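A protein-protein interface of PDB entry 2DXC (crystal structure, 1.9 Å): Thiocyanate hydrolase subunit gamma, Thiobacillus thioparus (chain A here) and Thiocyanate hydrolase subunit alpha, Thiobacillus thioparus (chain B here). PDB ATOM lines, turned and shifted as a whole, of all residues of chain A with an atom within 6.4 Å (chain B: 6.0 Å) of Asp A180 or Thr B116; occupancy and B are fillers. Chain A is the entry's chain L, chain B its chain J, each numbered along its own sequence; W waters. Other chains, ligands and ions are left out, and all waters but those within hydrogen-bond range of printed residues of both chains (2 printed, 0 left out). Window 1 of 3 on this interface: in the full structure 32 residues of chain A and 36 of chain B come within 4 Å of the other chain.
Thr A129 touches Met B57. OH of Tyr B59 touches CG1 of Val A156, 3.9 Å away. Leu B114 touches Val A156. CA of Leu B114 touches O of Val A178 (3.2 Å). Ala A179 touches Glu B115. OD2 of Asp A180 touches CE of Met B57, 3.5 Å away. Ile B118 touches Asn A182 (CD1 to ND2, 3.9 Å).
The backbone carbonyl oxygen (O) of Tyr B92 sits at hydrogen-bond distance from the backbone NH (N) of Ile B118. The side-chain carboxylate (OE2) of Glu B115 sits at hydrogen-bond distance from the side-chain hydroxyl (OG) of Ser B93 (2.6 Å). The backbone NH of Ile B94 sits at hydrogen-bond distance from the backbone carbonyl oxygen of Thr B116 (2.8 Å). N of Phe B96 is in hydrogen-bond range of O of Leu B114, 2.8 Å away. The backbone carbonyl oxygen (O) of Ala A179 sits at hydrogen-bond distance from the backbone NH (N) of Val A127 (3.0 Å). OG1 of Thr A129 lies within hydrogen-bond range of OD2 of Asp A180 (2.7 Å).
Printed residues of chain B within 4 Å of Ala A179: Glu B115. Asp A180 touches just these residues of chain B: Met B57 (3.5 Å), Tyr B59 (2.6 Å), Glu B115 (2.9 Å) and Thr B116 (3.0 Å). Printed residues of chain A within 4 Å of Tyr B59: Val A156 (3.9 Å) and Asp A180 (2.6 Å). The nearest residue of chain B that does not touch Asp A180 is Glu B117 (4.5 Å). The nearest printed residue of chain B that does not touch Asn A182 is Glu B115 (6.2 Å).
Of the 13 printed residues of chain B, 7 touch a printed residue of chain A. Printed residues of chain B that touch a printed residue of chain A: Met B57, Tyr B59, Leu B114, Glu B115, Thr B116, Glu B117 and Ile B118. Hydrophobic or aromatic side chains of chain B that line the printed part of chain A: Met B57, Tyr B59, Leu B114 and Ile B118. Of the 15 printed residues of chain A, 8 touch a printed residue of chain B. Hydrophobic or aromatic side chains of chain A within 4 Å of the printed part of chain B: Val A156. Among the printed residues, no Asp or Glu carboxylate lies within 4 Å of a Lys or Arg side-chain nitrogen of the other chain.
Water W2 lies within hydrogen-bond range of OH of Tyr A187 (2.6 Å), OE2 of Glu B117 (2.7 Å) and OG of Ser B93 (2.7 Å). Water W1 lies within hydrogen-bond range of the backbone NH (N) of Gln A183, the backbone carbonyl oxygen (O) of Thr A185, the side-chain carboxylate (OE1) of Glu B117 and the backbone NH (N) of Asn A182.
The side-chain sulfur (SD) of Met B57 sits at hydrogen-bond distance from the side-chain amide nitrogen (ND2) of Asn A182 (3.5 Å). OH of Tyr B59 lies within hydrogen-bond range of OD2 of Asp A180, 2.6 Å away. The backbone NH of Glu B115 is in hydrogen-bond range of the backbone carbonyl oxygen of Val A178, 2.8 Å away. The backbone NH (N) of Asp A180 sits at hydrogen-bond distance from the backbone carbonyl oxygen (O) of Glu B115, 2.9 Å away. OG1 of Thr B116 lies within hydrogen-bond range of O of Asp A180, 3.0 Å away. OG1 of Thr B116 lies within hydrogen-bond range of OD1 of Asn A182, at 2.8 Å. The backbone carbonyl oxygen of Glu B117 lies within hydrogen-bond range of the side-chain amide nitrogen of Asn A182 (2.7 Å). O of Glu B117 is in hydrogen-bond range of NE2 of Gln A183. The side-chain hydroxyl (OG1) of Thr A185 lies within hydrogen-bond range of the side-chain carboxylate (OE2) of Glu B117, 2.5 Å away.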
ATOM      1  N   VAL A 125     -35.411   0.260  -4.853  1.00  0.00           N
ATOM      2  CA  VAL A 125     -36.666   0.010  -4.151  1.00  0.00           C
ATOM      3  C   VAL A 125     -36.367   0.420  -2.707  1.00  0.00           C
ATOM      4  O   VAL A 125     -35.292   0.125  -2.179  1.00  0.00           O
ATOM      5  CB  VAL A 125     -37.131  -1.464  -4.249  1.00  0.00           C
ATOM      6  CG1 VAL A 125     -36.135  -2.394  -3.584  1.00  0.00           C
ATOM      7  CG2 VAL A 125     -38.515  -1.593  -3.625  1.00  0.00           C
ATOM      8  N   VAL A 126     -37.309   1.115  -2.079  1.00  0.00           N
ATOM      9  CA  VAL A 126     -37.101   1.641  -0.734  1.00  0.00           C
ATOM     10  C   VAL A 126     -37.932   1.034   0.394  1.00  0.00           C
ATOM     11  O   VAL A 126     -39.072   0.614   0.192  1.00  0.00           O
ATOM     12  CB  VAL A 126     -37.343   3.173  -0.748  1.00  0.00           C
ATOM     13  CG1 VAL A 126     -37.010   3.783   0.609  1.00  0.00           C
ATOM     14  CG2 VAL A 126     -36.516   3.813  -1.862  1.00  0.00           C
ATOM     15  N   VAL A 127     -37.346   1.016   1.591  1.00  0.00           N
ATOM     16  CA  VAL A 127     -38.004   0.495   2.784  1.00  0.00           C
ATOM     17  C   VAL A 127     -37.371   1.119   4.023  1.00  0.00           C
ATOM     18  O   VAL A 127     -36.303   1.725   3.947  1.00  0.00           O
ATOM     19  CB  VAL A 127     -37.837  -1.050   2.903  1.00  0.00           C
ATOM     20  CG1 VAL A 127     -36.363  -1.403   3.096  1.00  0.00           C
ATOM     21  CG2 VAL A 127     -38.651  -1.585   4.080  1.00  0.00           C
ATOM     22  N   CYS A 128     -38.054   0.989   5.157  1.00  0.00           N
ATOM     23  CA  CYS A 128     -37.538   1.448   6.443  1.00  0.00           C
ATOM     24  C   CYS A 128     -37.722   0.230   7.329  1.00  0.00           C
ATOM     25  O   CYS A 128     -38.796   0.022   7.892  1.00  0.00           O
ATOM     26  CB  CYS A 128     -38.343   2.618   7.022  1.00  0.00           C
ATOM     27  SG  CYS A 128     -37.791   3.090   8.713  1.00  0.00           S
ATOM     28  N   THR A 129     -36.683  -0.589   7.441  1.00  0.00           N
ATOM     29  CA  THR A 129     -36.784  -1.799   8.250  1.00  0.00           C
ATOM     30  C   THR A 129     -37.058  -1.519   9.724  1.00  0.00           C
ATOM     31  O   THR A 129     -37.714  -2.315  10.399  1.00  0.00           O
ATOM     32  CB  THR A 129     -35.511  -2.666   8.132  1.00  0.00           C
ATOM     33  OG1 THR A 129     -34.382  -1.956   8.657  1.00  0.00           O
ATOM     34  CG2 THR A 129     -35.250  -3.010   6.675  1.00  0.00           C
ATOM     35  N   LEU A 130     -36.572  -0.386  10.221  1.00  0.00           N
ATOM     36  CA  LEU A 130     -36.768  -0.033  11.626  1.00  0.00           C
ATOM     37  C   LEU A 130     -38.168   0.489  11.927  1.00  0.00           C
ATOM     38  O   LEU A 130     -38.626   0.438  13.069  1.00  0.00           O
ATOM     39  CB  LEU A 130     -35.723   1.005  12.054  1.00  0.00           C
ATOM     40  CG  LEU A 130     -34.275   0.508  11.938  1.00  0.00           C
ATOM     41  CD1 LEU A 130     -33.303   1.597  12.382  1.00  0.00           C
ATOM     42  CD2 LEU A 130     -34.112  -0.738  12.797  1.00  0.00           C
ATOM     43  N   VAL A 156     -35.329  -6.316   2.255  1.00  0.00           N
ATOM     44  CA  VAL A 156     -33.871  -6.204   2.238  1.00  0.00           C
ATOM     45  C   VAL A 156     -33.149  -7.509   1.925  1.00  0.00           C
ATOM     46  O   VAL A 156     -32.027  -7.488   1.413  1.00  0.00           O
ATOM     47  CB  VAL A 156     -33.306  -5.664   3.585  1.00  0.00           C
ATOM     48  CG1 VAL A 156     -33.793  -4.249   3.824  1.00  0.00           C
ATOM     49  CG2 VAL A 156     -33.707  -6.581   4.739  1.00  0.00           C
ATOM     50  N   VAL A 178     -31.604  -2.096  -2.770  1.00  0.00           N
ATOM     51  CA  VAL A 178     -32.608  -1.805  -1.762  1.00  0.00           C
ATOM     52  C   VAL A 178     -32.030  -0.703  -0.884  1.00  0.00           C
ATOM     53  O   VAL A 178     -30.900  -0.814  -0.410  1.00  0.00           O
ATOM     54  CB  VAL A 178     -32.914  -3.023  -0.865  1.00  0.00           C
ATOM     55  CG1 VAL A 178     -33.863  -2.608   0.256  1.00  0.00           C
ATOM     56  CG2 VAL A 178     -33.538  -4.140  -1.689  1.00  0.00           C
ATOM     57  N   ALA A 179     -32.795   0.366  -0.690  1.00  0.00           N
ATOM     58  CA  ALA A 179     -32.358   1.474   0.151  1.00  0.00           C
ATOM     59  C   ALA A 179     -33.115   1.384   1.467  1.00  0.00           C
ATOM     60  O   ALA A 179     -34.344   1.415   1.480  1.00  0.00           O
ATOM     61  CB  ALA A 179     -32.653   2.815  -0.533  1.00  0.00           C
ATOM     62  N   ASP A 180     -32.385   1.260   2.571  1.00  0.00           N
ATOM     63  CA  ASP A 180     -33.014   1.177   3.886  1.00  0.00           C
ATOM     64  C   ASP A 180     -32.905   2.551   4.552  1.00  0.00           C
ATOM     65  O   ASP A 180     -31.815   2.963   4.959  1.00  0.00           O
ATOM     66  CB  ASP A 180     -32.314   0.110   4.736  1.00  0.00           C
ATOM     67  CG  ASP A 180     -33.099  -0.254   5.986  1.00  0.00           C
ATOM     68  OD1 ASP A 180     -34.057   0.470   6.327  1.00  0.00           O
ATOM     69  OD2 ASP A 180     -32.749  -1.261   6.637  1.00  0.00           O
ATOM     70  N   SER A 181     -34.034   3.256   4.647  1.00  0.00           N
ATOM     71  CA  SER A 181     -34.085   4.594   5.244  1.00  0.00           C
ATOM     72  C   SER A 181     -34.059   4.494   6.766  1.00  0.00           C
ATOM     73  O   SER A 181     -35.091   4.652   7.412  1.00  0.00           O
ATOM     74  CB  SER A 181     -35.376   5.312   4.828  1.00  0.00           C
ATOM     75  OG  SER A 181     -35.728   5.014   3.491  1.00  0.00           O
ATOM     76  N   ASN A 182     -32.880   4.270   7.339  1.00  0.00           N
ATOM     77  CA  ASN A 182     -32.756   4.102   8.785  1.00  0.00           C
ATOM     78  C   ASN A 182     -32.325   5.324   9.592  1.00  0.00           C
ATOM     79  O   ASN A 182     -32.429   5.318  10.817  1.00  0.00           O
ATOM     80  CB  ASN A 182     -31.790   2.958   9.073  1.00  0.00           C
ATOM     81  CG  ASN A 182     -30.382   3.277   8.636  1.00  0.00           C
ATOM     82  OD1 ASN A 182     -30.176   3.949   7.620  1.00  0.00           O
ATOM     83  ND2 ASN A 182     -29.399   2.794   9.389  1.00  0.00           N
ATOM     84  N   GLN A 183     -31.821   6.361   8.933  1.00  0.00           N
ATOM     85  CA  GLN A 183     -31.403   7.551   9.669  1.00  0.00           C
ATOM     86  C   GLN A 183     -32.242   8.754   9.229  1.00  0.00           C
ATOM     87  O   GLN A 183     -33.454   8.633   9.083  1.00  0.00           O
ATOM     88  CB  GLN A 183     -29.909   7.815   9.461  1.00  0.00           C
ATOM     89  CG  GLN A 183     -28.976   6.635   9.815  1.00  0.00           C
ATOM     90  CD  GLN A 183     -28.970   6.242  11.300  1.00  0.00           C
ATOM     91  OE1 GLN A 183     -29.446   6.979  12.166  1.00  0.00           O
ATOM     92  NE2 GLN A 183     -28.405   5.074  11.590  1.00  0.00           N
ATOM     93  N   THR A 185     -32.124  10.431   6.282  1.00  0.00           N
ATOM     94  CA  THR A 185     -32.356  10.568   4.851  1.00  0.00           C
ATOM     95  C   THR A 185     -33.648   9.860   4.449  1.00  0.00           C
ATOM     96  O   THR A 185     -33.975   8.791   4.965  1.00  0.00           O
ATOM     97  CB  THR A 185     -31.191   9.973   4.031  1.00  0.00           C
ATOM     98  OG1 THR A 185     -30.046  10.826   4.145  1.00  0.00           O
ATOM     99  CG2 THR A 185     -31.575   9.835   2.556  1.00  0.00           C
ATOM    100  N   TYR A 187     -35.914   8.826   0.853  1.00  0.00           N
ATOM    101  CA  TYR A 187     -35.682   8.663  -0.581  1.00  0.00           C
ATOM    102  C   TYR A 187     -36.928   8.598  -1.450  1.00  0.00           C
ATOM    103  O   TYR A 187     -38.005   8.242  -0.990  1.00  0.00           O
ATOM    104  CB  TYR A 187     -34.938   7.348  -0.858  1.00  0.00           C
ATOM    105  CG  TYR A 187     -33.694   7.062  -0.047  1.00  0.00           C
ATOM    106  CD1 TYR A 187     -32.441   7.505  -0.470  1.00  0.00           C
ATOM    107  CD2 TYR A 187     -33.762   6.287   1.112  1.00  0.00           C
ATOM    108  CE1 TYR A 187     -31.283   7.174   0.239  1.00  0.00           C
ATOM    109  CE2 TYR A 187     -32.612   5.952   1.826  1.00  0.00           C
ATOM    110  CZ  TYR A 187     -31.379   6.395   1.385  1.00  0.00           C
ATOM    111  OH  TYR A 187     -30.245   6.049   2.084  1.00  0.00           O
ATOM    112  N   MET B  57     -28.874  -1.515  12.050  1.00  0.00           N
ATOM    113  CA  MET B  57     -29.471  -2.844  11.985  1.00  0.00           C
ATOM    114  C   MET B  57     -28.529  -3.999  12.284  1.00  0.00           C
ATOM    115  O   MET B  57     -27.360  -3.986  11.903  1.00  0.00           O
ATOM    116  CB  MET B  57     -30.122  -3.070  10.616  1.00  0.00           C
ATOM    117  CG  MET B  57     -31.242  -2.090  10.257  1.00  0.00           C
ATOM    118  SD  MET B  57     -30.661  -0.419   9.880  1.00  0.00           S
ATOM    119  CE  MET B  57     -29.753  -0.714   8.362  1.00  0.00           C
ATOM    120  N   TYR B  59     -28.586  -6.893  10.987  1.00  0.00           N
ATOM    121  CA  TYR B  59     -28.181  -7.553   9.747  1.00  0.00           C
ATOM    122  C   TYR B  59     -26.921  -6.996   9.081  1.00  0.00           C
ATOM    123  O   TYR B  59     -26.359  -7.637   8.189  1.00  0.00           O
ATOM    124  CB  TYR B  59     -29.355  -7.602   8.741  1.00  0.00           C
ATOM    125  CG  TYR B  59     -29.707  -6.316   8.004  1.00  0.00           C
ATOM    126  CD1 TYR B  59     -28.906  -5.835   6.968  1.00  0.00           C
ATOM    127  CD2 TYR B  59     -30.876  -5.618   8.305  1.00  0.00           C
ATOM    128  CE1 TYR B  59     -29.269  -4.685   6.244  1.00  0.00           C
ATOM    129  CE2 TYR B  59     -31.245  -4.474   7.593  1.00  0.00           C
ATOM    130  CZ  TYR B  59     -30.439  -4.013   6.565  1.00  0.00           C
ATOM    131  OH  TYR B  59     -30.802  -2.883   5.863  1.00  0.00           O
ATOM    132  N   THR B  60     -26.463  -5.822   9.516  1.00  0.00           N
ATOM    133  CA  THR B  60     -25.250  -5.231   8.942  1.00  0.00           C
ATOM    134  C   THR B  60     -23.986  -5.487   9.767  1.00  0.00           C
ATOM    135  O   THR B  60     -22.871  -5.299   9.268  1.00  0.00           O
ATOM    136  CB  THR B  60     -25.358  -3.696   8.796  1.00  0.00           C
ATOM    137  OG1 THR B  60     -25.415  -3.101  10.100  1.00  0.00           O
ATOM    138  CG2 THR B  60     -26.597  -3.309   8.003  1.00  0.00           C
ATOM    139  N   TYR B  92     -22.562   8.306   7.108  1.00  0.00           N
ATOM    140  CA  TYR B  92     -22.145   7.831   5.795  1.00  0.00           C
ATOM    141  C   TYR B  92     -23.177   6.914   5.157  1.00  0.00           C
ATOM    142  O   TYR B  92     -23.839   6.140   5.846  1.00  0.00           O
ATOM    143  CB  TYR B  92     -20.837   7.047   5.924  1.00  0.00           C
ATOM    144  CG  TYR B  92     -19.700   7.796   6.581  1.00  0.00           C
ATOM    145  CD1 TYR B  92     -18.682   8.363   5.814  1.00  0.00           C
ATOM    146  CD2 TYR B  92     -19.627   7.921   7.967  1.00  0.00           C
ATOM    147  CE1 TYR B  92     -17.613   9.030   6.411  1.00  0.00           C
ATOM    148  CE2 TYR B  92     -18.561   8.591   8.577  1.00  0.00           C
ATOM    149  CZ  TYR B  92     -17.557   9.143   7.789  1.00  0.00           C
ATOM    150  OH  TYR B  92     -16.499   9.806   8.372  1.00  0.00           O
ATOM    151  N   SER B  93     -23.313   7.002   3.839  1.00  0.00           N
ATOM    152  CA  SER B  93     -24.223   6.121   3.130  1.00  0.00           C
ATOM    153  C   SER B  93     -23.299   5.003   2.655  1.00  0.00           C
ATOM    154  O   SER B  93     -22.292   5.260   1.979  1.00  0.00           O
ATOM    155  CB  SER B  93     -24.873   6.827   1.940  1.00  0.00           C
ATOM    156  OG  SER B  93     -26.007   6.096   1.496  1.00  0.00           O
ATOM    157  N   ILE B  94     -23.626   3.769   3.028  1.00  0.00           N
ATOM    158  CA  ILE B  94     -22.805   2.614   2.675  1.00  0.00           C
ATOM    159  C   ILE B  94     -23.529   1.601   1.796  1.00  0.00           C
ATOM    160  O   ILE B  94     -24.694   1.276   2.037  1.00  0.00           O
ATOM    161  CB  ILE B  94     -22.309   1.884   3.953  1.00  0.00           C
ATOM    162  CG1 ILE B  94     -21.462   2.838   4.805  1.00  0.00           C
ATOM    163  CG2 ILE B  94     -21.475   0.673   3.581  1.00  0.00           C
ATOM    164  CD1 ILE B  94     -22.262   3.744   5.688  1.00  0.00           C
ATOM    165  N   VAL B  95     -22.830   1.103   0.779  1.00  0.00           N
ATOM    166  CA  VAL B  95     -23.397   0.111  -0.126  1.00  0.00           C
ATOM    167  C   VAL B  95     -22.775  -1.253   0.150  1.00  0.00           C
ATOM    168  O   VAL B  95     -21.549  -1.409   0.149  1.00  0.00           O
ATOM    169  CB  VAL B  95     -23.154   0.489  -1.603  1.00  0.00           C
ATOM    170  CG1 VAL B  95     -23.540  -0.677  -2.517  1.00  0.00           C
ATOM    171  CG2 VAL B  95     -23.979   1.721  -1.961  1.00  0.00           C
ATOM    172  N   PHE B  96     -23.640  -2.233   0.393  1.00  0.00           N
ATOM    173  CA  PHE B  96     -23.234  -3.603   0.682  1.00  0.00           C
ATOM    174  C   PHE B  96     -23.634  -4.523  -0.466  1.00  0.00           C
ATOM    175  O   PHE B  96     -24.695  -4.343  -1.066  1.00  0.00           O
ATOM    176  CB  PHE B  96     -23.949  -4.115   1.935  1.00  0.00           C
ATOM    177  CG  PHE B  96     -23.586  -3.389   3.197  1.00  0.00           C
ATOM    178  CD1 PHE B  96     -22.451  -3.743   3.915  1.00  0.00           C
ATOM    179  CD2 PHE B  96     -24.405  -2.376   3.691  1.00  0.00           C
ATOM    180  CE1 PHE B  96     -22.134  -3.104   5.113  1.00  0.00           C
ATOM    181  CE2 PHE B  96     -24.099  -1.729   4.887  1.00  0.00           C
ATOM    182  CZ  PHE B  96     -22.962  -2.094   5.600  1.00  0.00           C
ATOM    183  N   LEU B 114     -27.419  -3.315  -1.251  1.00  0.00           N
ATOM    184  CA  LEU B 114     -28.256  -2.693  -0.237  1.00  0.00           C
ATOM    185  C   LEU B 114     -27.507  -1.459   0.248  1.00  0.00           C
ATOM    186  O   LEU B 114     -26.317  -1.536   0.562  1.00  0.00           O
ATOM    187  CB  LEU B 114     -28.505  -3.653   0.932  1.00  0.00           C
ATOM    188  CG  LEU B 114     -29.371  -3.085   2.067  1.00  0.00           C
ATOM    189  CD1 LEU B 114     -30.218  -4.186   2.674  1.00  0.00           C
ATOM    190  CD2 LEU B 114     -28.489  -2.431   3.126  1.00  0.00           C
ATOM    191  N   GLU B 115     -28.198  -0.323   0.281  1.00  0.00           N
ATOM    192  CA  GLU B 115     -27.597   0.929   0.728  1.00  0.00           C
ATOM    193  C   GLU B 115     -28.317   1.433   1.972  1.00  0.00           C
ATOM    194  O   GLU B 115     -29.549   1.448   2.032  1.00  0.00           O
ATOM    195  CB  GLU B 115     -27.672   1.993  -0.379  1.00  0.00           C
ATOM    196  CG  GLU B 115     -26.911   3.280  -0.049  1.00  0.00           C
ATOM    197  CD  GLU B 115     -26.918   4.299  -1.184  1.00  0.00           C
ATOM    198  OE1 GLU B 115     -27.252   3.928  -2.330  1.00  0.00           O
ATOM    199  OE2 GLU B 115     -26.576   5.474  -0.928  1.00  0.00           O
ATOM    200  N   THR B 116     -27.548   1.848   2.969  1.00  0.00           N
ATOM    201  CA  THR B 116     -28.136   2.350   4.199  1.00  0.00           C
ATOM    202  C   THR B 116     -27.135   3.288   4.879  1.00  0.00           C
ATOM    203  O   THR B 116     -25.957   3.313   4.508  1.00  0.00           O
ATOM    204  CB  THR B 116     -28.533   1.166   5.116  1.00  0.00           C
ATOM    205  OG1 THR B 116     -29.365   1.637   6.180  1.00  0.00           O
ATOM    206  CG2 THR B 116     -27.299   0.477   5.681  1.00  0.00           C
ATOM    207  N   GLU B 117     -27.596   4.062   5.859  1.00  0.00           N
ATOM    208  CA  GLU B 117     -26.725   5.019   6.541  1.00  0.00           C
ATOM    209  C   GLU B 117     -26.294   4.590   7.940  1.00  0.00           C
ATOM    210  O   GLU B 117     -27.087   4.050   8.712  1.00  0.00           O
ATOM    211  CB  GLU B 117     -27.410   6.395   6.593  1.00  0.00           C
ATOM    212  CG  GLU B 117     -27.772   6.927   5.201  1.00  0.00           C
ATOM    213  CD  GLU B 117     -28.312   8.352   5.207  1.00  0.00           C
ATOM    214  OE1 GLU B 117     -28.798   8.806   6.264  1.00  0.00           O
ATOM    215  OE2 GLU B 117     -28.264   9.008   4.143  1.00  0.00           O
ATOM    216  N   ILE B 118     -25.028   4.843   8.259  1.00  0.00           N
ATOM    217  CA  ILE B 118     -24.464   4.479   9.554  1.00  0.00           C
ATOM    218  C   ILE B 118     -23.550   5.586  10.086  1.00  0.00           C
ATOM    219  O   ILE B 118     -22.721   6.130   9.346  1.00  0.00           O
ATOM    220  CB  ILE B 118     -23.635   3.180   9.445  1.00  0.00           C
ATOM    221  CG1 ILE B 118     -24.512   2.049   8.896  1.00  0.00           C
ATOM    222  CG2 ILE B 118     -23.085   2.791  10.803  1.00  0.00           C
ATOM    223  CD1 ILE B 118     -25.715   1.684   9.787  1.00  0.00           C
HETATM  224  O   HOH W   1     -31.874   7.389   6.360  1.00  0.00           O
HETATM  225  O   HOH W   2     -28.201   7.670   1.809  1.00  0.00           O
